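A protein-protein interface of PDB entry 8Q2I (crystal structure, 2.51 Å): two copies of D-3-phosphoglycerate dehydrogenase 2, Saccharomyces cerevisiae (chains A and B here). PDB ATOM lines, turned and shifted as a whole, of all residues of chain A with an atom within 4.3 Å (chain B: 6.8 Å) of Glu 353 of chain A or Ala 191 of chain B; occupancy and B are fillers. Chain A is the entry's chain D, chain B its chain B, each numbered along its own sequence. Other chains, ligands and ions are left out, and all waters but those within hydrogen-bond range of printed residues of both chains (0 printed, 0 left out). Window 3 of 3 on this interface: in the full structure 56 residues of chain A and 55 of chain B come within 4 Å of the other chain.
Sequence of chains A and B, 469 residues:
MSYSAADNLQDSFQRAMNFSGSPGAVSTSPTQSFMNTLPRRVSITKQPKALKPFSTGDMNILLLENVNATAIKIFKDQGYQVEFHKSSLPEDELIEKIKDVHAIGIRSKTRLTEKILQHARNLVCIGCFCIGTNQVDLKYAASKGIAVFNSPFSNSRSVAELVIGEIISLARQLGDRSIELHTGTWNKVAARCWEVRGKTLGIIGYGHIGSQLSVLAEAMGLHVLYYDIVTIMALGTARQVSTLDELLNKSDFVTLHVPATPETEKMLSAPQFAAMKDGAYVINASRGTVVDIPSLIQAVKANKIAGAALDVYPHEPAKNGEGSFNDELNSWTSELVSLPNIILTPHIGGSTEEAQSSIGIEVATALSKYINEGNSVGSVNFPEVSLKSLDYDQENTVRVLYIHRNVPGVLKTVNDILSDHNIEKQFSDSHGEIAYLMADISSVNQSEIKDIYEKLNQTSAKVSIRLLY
The side-chain carboxylate of Glu 354 of chain A sits at hydrogen-bond distance from the backbone NH of Glu 195 of chain B, 2.9 Å away.
The backbone NH (N) of Glu 353 of chain A is in hydrogen-bond range of the backbone carbonyl oxygen (O) of Cys 193 of chain B, 3.1 Å away.
The side-chain carboxylate (OE2) of Glu 353 of chain A lies within hydrogen-bond range of the backbone NH (N) of Arg 192 of chain B (3.1 Å).
The backbone carbonyl oxygen (O) of Arg 192 of chain B sits at hydrogen-bond distance from the indole nitrogen (NE1) of Trp 194 of chain B (3.0 Å).
O of Ala 191 of chain B is in hydrogen-bond range of SG of Cys 193 of chain B (3.8 Å).
O of Val 189 of chain B sits at hydrogen-bond distance from SG of Cys 193 of chain B (3.7 Å).
The side-chain sulfur of Cys 193 of chain B is in hydrogen-bond range of the side-chain amide nitrogen of Gln 173 of chain B (3.5 Å).
The side-chain hydroxyl (OG1) of Thr 352 of chain A is in hydrogen-bond range of the backbone NH (N) of Ala 355 of chain A (3.1 Å).
CB of Ala 190 of chain B touches N of Thr 352 of chain A, at 3.9 Å.
Thr 352 of chain A touches Cys 193 of chain B (CA to O, 3.6 Å).
Trp 194 of chain B touches Thr 352 of chain A.
Glu 195 of chain B touches Thr 352 of chain A.
Ala 190 of chain B touches Glu 353 of chain A.
Ala 191 of chain B touches Glu 353 of chain A (CA to OE2, 3.7 Å).
Trp 194 of chain B touches Glu 353 of chain A.
Glu 354 of chain A touches Trp 194 of chain B.
Glu 195 of chain B touches Ala 355 of chain A (OE2 to N, 3.99 Å).
Of the printed residues of chain B, Thr 352 of chain A touches Ala 190 (3.9 Å), Cys 193 (3.6 Å), Trp 194 (3.95 Å) and Glu 195 (3.6 Å).
Of chain B, only Ala 190, Ala 191, Arg 192, Cys 193 and Trp 194 come within 4 Å of Glu 353 of chain A.
Gln 356 of chain A touches none of the printed residues of chain B.
Ser 357 of chain A touches none of the printed residues of chain B.
Of the printed residues of chain A, Ala 190 of chain B touches Thr 352 (3.9 Å) and Glu 353 (3.5 Å).
Of chain A, only Glu 353 comes within 4 Å of Ala 191 of chain B.
Of the printed residues of chain A, Arg 192 of chain B touches Glu 353.
Printed residues of chain A within 4 Å of Trp 194 of chain B: Thr 352, Glu 353 and Glu 354.
Printed residues of chain A within 4 Å of Glu 195 of chain B: Thr 352, Glu 354 and Ala 355.
The nearest printed residue of chain A that does not touch Ala 190 of chain B is Gln 356 of chain A (4.3 Å).
Printed residues of chain A that touch a printed residue of chain B: Thr 352, Glu 353, Glu 354 and Ala 355.
Along chain A the printed residues that touch a printed residue of chain B span positions 352 to 355.
Among the printed residues, 12 pairs touch across the chains.
Among the printed residues, no Asp or Glu carboxylate lies within 4 Å of a Lys or Arg side-chain nitrogen of the other chain.
No position is printed for both chains.
Of the 12 pairs that touch across the chains among the printed residues, none has its exchanged pair printed and touching as well.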
ATOM      1  N   THR A 352      -7.614  20.369 -16.254  1.00  0.00           N
ATOM      2  CA  THR A 352      -8.926  20.761 -15.757  1.00  0.00           C
ATOM      3  C   THR A 352      -8.795  21.845 -14.688  1.00  0.00           C
ATOM      4  O   THR A 352      -7.742  22.073 -14.103  1.00  0.00           O
ATOM      5  CB  THR A 352      -9.697  19.562 -15.192  1.00  0.00           C
ATOM      6  OG1 THR A 352      -9.061  19.027 -14.037  1.00  0.00           O
ATOM      7  CG2 THR A 352      -9.789  18.441 -16.191  1.00  0.00           C
ATOM      8  N   GLU A 353      -9.907  22.502 -14.428  1.00  0.00           N
ATOM      9  CA  GLU A 353     -10.005  23.468 -13.350  1.00  0.00           C
ATOM     10  C   GLU A 353      -9.779  22.773 -12.014  1.00  0.00           C
ATOM     11  O   GLU A 353      -9.166  23.353 -11.126  1.00  0.00           O
ATOM     12  CB  GLU A 353     -11.363  24.137 -13.429  1.00  0.00           C
ATOM     13  CG  GLU A 353     -11.528  25.019 -14.664  1.00  0.00           C
ATOM     14  CD  GLU A 353     -11.109  26.464 -14.463  1.00  0.00           C
ATOM     15  OE1 GLU A 353     -10.478  26.788 -13.434  1.00  0.00           O
ATOM     16  OE2 GLU A 353     -11.468  27.307 -15.310  1.00  0.00           O
ATOM     17  N   GLU A 354     -10.237  21.527 -11.852  1.00  0.00           N
ATOM     18  CA  GLU A 354     -10.150  20.857 -10.560  1.00  0.00           C
ATOM     19  C   GLU A 354      -8.705  20.486 -10.267  1.00  0.00           C
ATOM     20  O   GLU A 354      -8.263  20.533  -9.131  1.00  0.00           O
ATOM     21  CB  GLU A 354     -11.017  19.593 -10.535  1.00  0.00           C
ATOM     22  CG  GLU A 354     -12.523  19.842 -10.433  1.00  0.00           C
ATOM     23  CD  GLU A 354     -13.225  20.462 -11.635  1.00  0.00           C
ATOM     24  OE1 GLU A 354     -12.659  20.418 -12.788  1.00  0.00           O
ATOM     25  OE2 GLU A 354     -14.341  21.031 -11.410  1.00  0.00           O
ATOM     26  N   ALA A 355      -7.986  20.069 -11.300  1.00  0.00           N
ATOM     27  CA  ALA A 355      -6.596  19.667 -11.170  1.00  0.00           C
ATOM     28  C   ALA A 355      -5.736  20.898 -10.881  1.00  0.00           C
ATOM     29  O   ALA A 355      -4.964  20.868  -9.949  1.00  0.00           O
ATOM     30  CB  ALA A 355      -6.138  18.934 -12.407  1.00  0.00           C
ATOM     31  N   GLN A 356      -5.866  21.963 -11.667  1.00  0.00           N
ATOM     32  CA  GLN A 356      -5.139  23.205 -11.448  1.00  0.00           C
ATOM     33  C   GLN A 356      -5.388  23.767 -10.048  1.00  0.00           C
ATOM     34  O   GLN A 356      -4.510  24.339  -9.423  1.00  0.00           O
ATOM     35  CB  GLN A 356      -5.544  24.234 -12.501  1.00  0.00           C
ATOM     36  CG  GLN A 356      -4.881  23.980 -13.840  1.00  0.00           C
ATOM     37  CD  GLN A 356      -3.389  24.092 -13.643  1.00  0.00           C
ATOM     38  OE1 GLN A 356      -2.855  25.153 -13.300  1.00  0.00           O
ATOM     39  NE2 GLN A 356      -2.711  22.964 -13.764  1.00  0.00           N
ATOM     40  N   SER A 357      -6.605  23.571  -9.568  1.00  0.00           N
ATOM     41  CA  SER A 357      -7.006  24.027  -8.258  1.00  0.00           C
ATOM     42  C   SER A 357      -6.390  23.157  -7.155  1.00  0.00           C
ATOM     43  O   SER A 357      -6.011  23.655  -6.107  1.00  0.00           O
ATOM     44  CB  SER A 357      -8.510  24.093  -8.203  1.00  0.00           C
ATOM     45  OG  SER A 357      -8.989  23.748  -6.917  1.00  0.00           O
ATOM     46  N   GLN B 173     -13.797  19.266 -23.852  1.00  0.00           N
ATOM     47  CA  GLN B 173     -13.697  19.726 -25.228  1.00  0.00           C
ATOM     48  C   GLN B 173     -12.855  18.776 -26.087  1.00  0.00           C
ATOM     49  O   GLN B 173     -12.120  19.231 -26.959  1.00  0.00           O
ATOM     50  CB  GLN B 173     -13.137  21.147 -25.246  1.00  0.00           C
ATOM     51  CG  GLN B 173     -13.924  22.158 -24.408  1.00  0.00           C
ATOM     52  CD  GLN B 173     -13.230  23.496 -24.229  1.00  0.00           C
ATOM     53  OE1 GLN B 173     -12.252  23.821 -24.886  1.00  0.00           O
ATOM     54  NE2 GLN B 173     -13.710  24.300 -23.301  1.00  0.00           N
ATOM     55  N   LYS B 188      -3.621  23.657 -25.956  1.00  0.00           N
ATOM     56  CA  LYS B 188      -3.819  23.110 -24.623  1.00  0.00           C
ATOM     57  C   LYS B 188      -4.630  24.093 -23.787  1.00  0.00           C
ATOM     58  O   LYS B 188      -4.234  25.240 -23.645  1.00  0.00           O
ATOM     59  CB  LYS B 188      -2.461  22.820 -23.992  1.00  0.00           C
ATOM     60  CG  LYS B 188      -2.452  22.047 -22.683  1.00  0.00           C
ATOM     61  CD  LYS B 188      -1.026  21.625 -22.335  1.00  0.00           C
ATOM     62  CE  LYS B 188      -0.862  21.177 -20.898  1.00  0.00           C
ATOM     63  NZ  LYS B 188       0.297  20.258 -20.769  1.00  0.00           N
ATOM     64  N   VAL B 189      -5.751  23.627 -23.220  1.00  0.00           N
ATOM     65  CA  VAL B 189      -6.742  24.461 -22.553  1.00  0.00           C
ATOM     66  C   VAL B 189      -7.207  23.733 -21.293  1.00  0.00           C
ATOM     67  O   VAL B 189      -7.706  22.614 -21.412  1.00  0.00           O
ATOM     68  CB  VAL B 189      -7.930  24.732 -23.502  1.00  0.00           C
ATOM     69  CG1 VAL B 189      -9.110  25.399 -22.804  1.00  0.00           C
ATOM     70  CG2 VAL B 189      -7.520  25.538 -24.735  1.00  0.00           C
ATOM     71  N   ALA B 190      -7.060  24.368 -20.106  1.00  0.00           N
ATOM     72  CA  ALA B 190      -7.684  23.888 -18.865  1.00  0.00           C
ATOM     73  C   ALA B 190      -8.913  24.717 -18.463  1.00  0.00           C
ATOM     74  O   ALA B 190      -9.695  24.278 -17.609  1.00  0.00           O
ATOM     75  CB  ALA B 190      -6.691  23.850 -17.735  1.00  0.00           C
ATOM     76  N   ALA B 191      -9.067  25.906 -19.081  1.00  0.00           N
ATOM     77  CA  ALA B 191     -10.065  26.906 -18.703  1.00  0.00           C
ATOM     78  C   ALA B 191     -11.469  26.414 -19.064  1.00  0.00           C
ATOM     79  O   ALA B 191     -11.786  26.201 -20.240  1.00  0.00           O
ATOM     80  CB  ALA B 191      -9.747  28.236 -19.353  1.00  0.00           C
ATOM     81  N   ARG B 192     -12.283  26.207 -18.038  1.00  0.00           N
ATOM     82  CA  ARG B 192     -13.679  25.776 -18.253  1.00  0.00           C
ATOM     83  C   ARG B 192     -13.674  24.354 -18.797  1.00  0.00           C
ATOM     84  O   ARG B 192     -14.608  24.006 -19.520  1.00  0.00           O
ATOM     85  CB  ARG B 192     -14.384  26.766 -19.180  1.00  0.00           C
ATOM     86  CG  ARG B 192     -14.363  28.207 -18.693  1.00  0.00           C
ATOM     87  CD  ARG B 192     -15.058  28.352 -17.357  1.00  0.00           C
ATOM     88  NE  ARG B 192     -15.002  29.724 -16.883  1.00  0.00           N
ATOM     89  CZ  ARG B 192     -15.523  30.145 -15.740  1.00  0.00           C
ATOM     90  NH1 ARG B 192     -16.148  29.296 -14.943  1.00  0.00           N
ATOM     91  NH2 ARG B 192     -15.415  31.416 -15.396  1.00  0.00           N
ATOM     92  N   CYS B 193     -12.646  23.585 -18.465  1.00  0.00           N
ATOM     93  CA  CYS B 193     -12.614  22.167 -18.872  1.00  0.00           C
ATOM     94  C   CYS B 193     -12.738  21.517 -17.505  1.00  0.00           C
ATOM     95  O   CYS B 193     -12.162  22.049 -16.567  1.00  0.00           O
ATOM     96  CB  CYS B 193     -11.377  21.842 -19.691  1.00  0.00           C
ATOM     97  SG  CYS B 193     -11.396  22.586 -21.336  1.00  0.00           S
ATOM     98  N   TRP B 194     -13.509  20.449 -17.378  1.00  0.00           N
ATOM     99  CA  TRP B 194     -13.813  19.988 -16.006  1.00  0.00           C
ATOM    100  C   TRP B 194     -13.713  18.505 -15.726  1.00  0.00           C
ATOM    101  O   TRP B 194     -13.824  17.714 -16.643  1.00  0.00           O
ATOM    102  CB  TRP B 194     -15.261  20.389 -15.683  1.00  0.00           C
ATOM    103  CG  TRP B 194     -15.686  21.753 -16.121  1.00  0.00           C
ATOM    104  CD1 TRP B 194     -16.264  22.092 -17.306  1.00  0.00           C
ATOM    105  CD2 TRP B 194     -15.595  22.964 -15.355  1.00  0.00           C
ATOM    106  NE1 TRP B 194     -16.519  23.433 -17.340  1.00  0.00           N
ATOM    107  CE2 TRP B 194     -16.120  23.995 -16.157  1.00  0.00           C
ATOM    108  CE3 TRP B 194     -15.109  23.278 -14.084  1.00  0.00           C
ATOM    109  CZ2 TRP B 194     -16.175  25.316 -15.724  1.00  0.00           C
ATOM    110  CZ3 TRP B 194     -15.165  24.583 -13.657  1.00  0.00           C
ATOM    111  CH2 TRP B 194     -15.690  25.586 -14.468  1.00  0.00           C
ATOM    112  N   GLU B 195     -13.497  18.189 -14.464  1.00  0.00           N
ATOM    113  CA  GLU B 195     -13.613  16.805 -14.016  1.00  0.00           C
ATOM    114  C   GLU B 195     -15.106  16.666 -13.754  1.00  0.00           C
ATOM    115  O   GLU B 195     -15.689  17.603 -13.216  1.00  0.00           O
ATOM    116  CB  GLU B 195     -12.856  16.587 -12.713  1.00  0.00           C
ATOM    117  CG  GLU B 195     -11.351  16.564 -12.839  1.00  0.00           C
ATOM    118  CD  GLU B 195     -10.664  16.258 -11.520  1.00  0.00           C
ATOM    119  OE1 GLU B 195     -11.372  15.934 -10.555  1.00  0.00           O
ATOM    120  OE2 GLU B 195      -9.432  16.350 -11.459  1.00  0.00           O
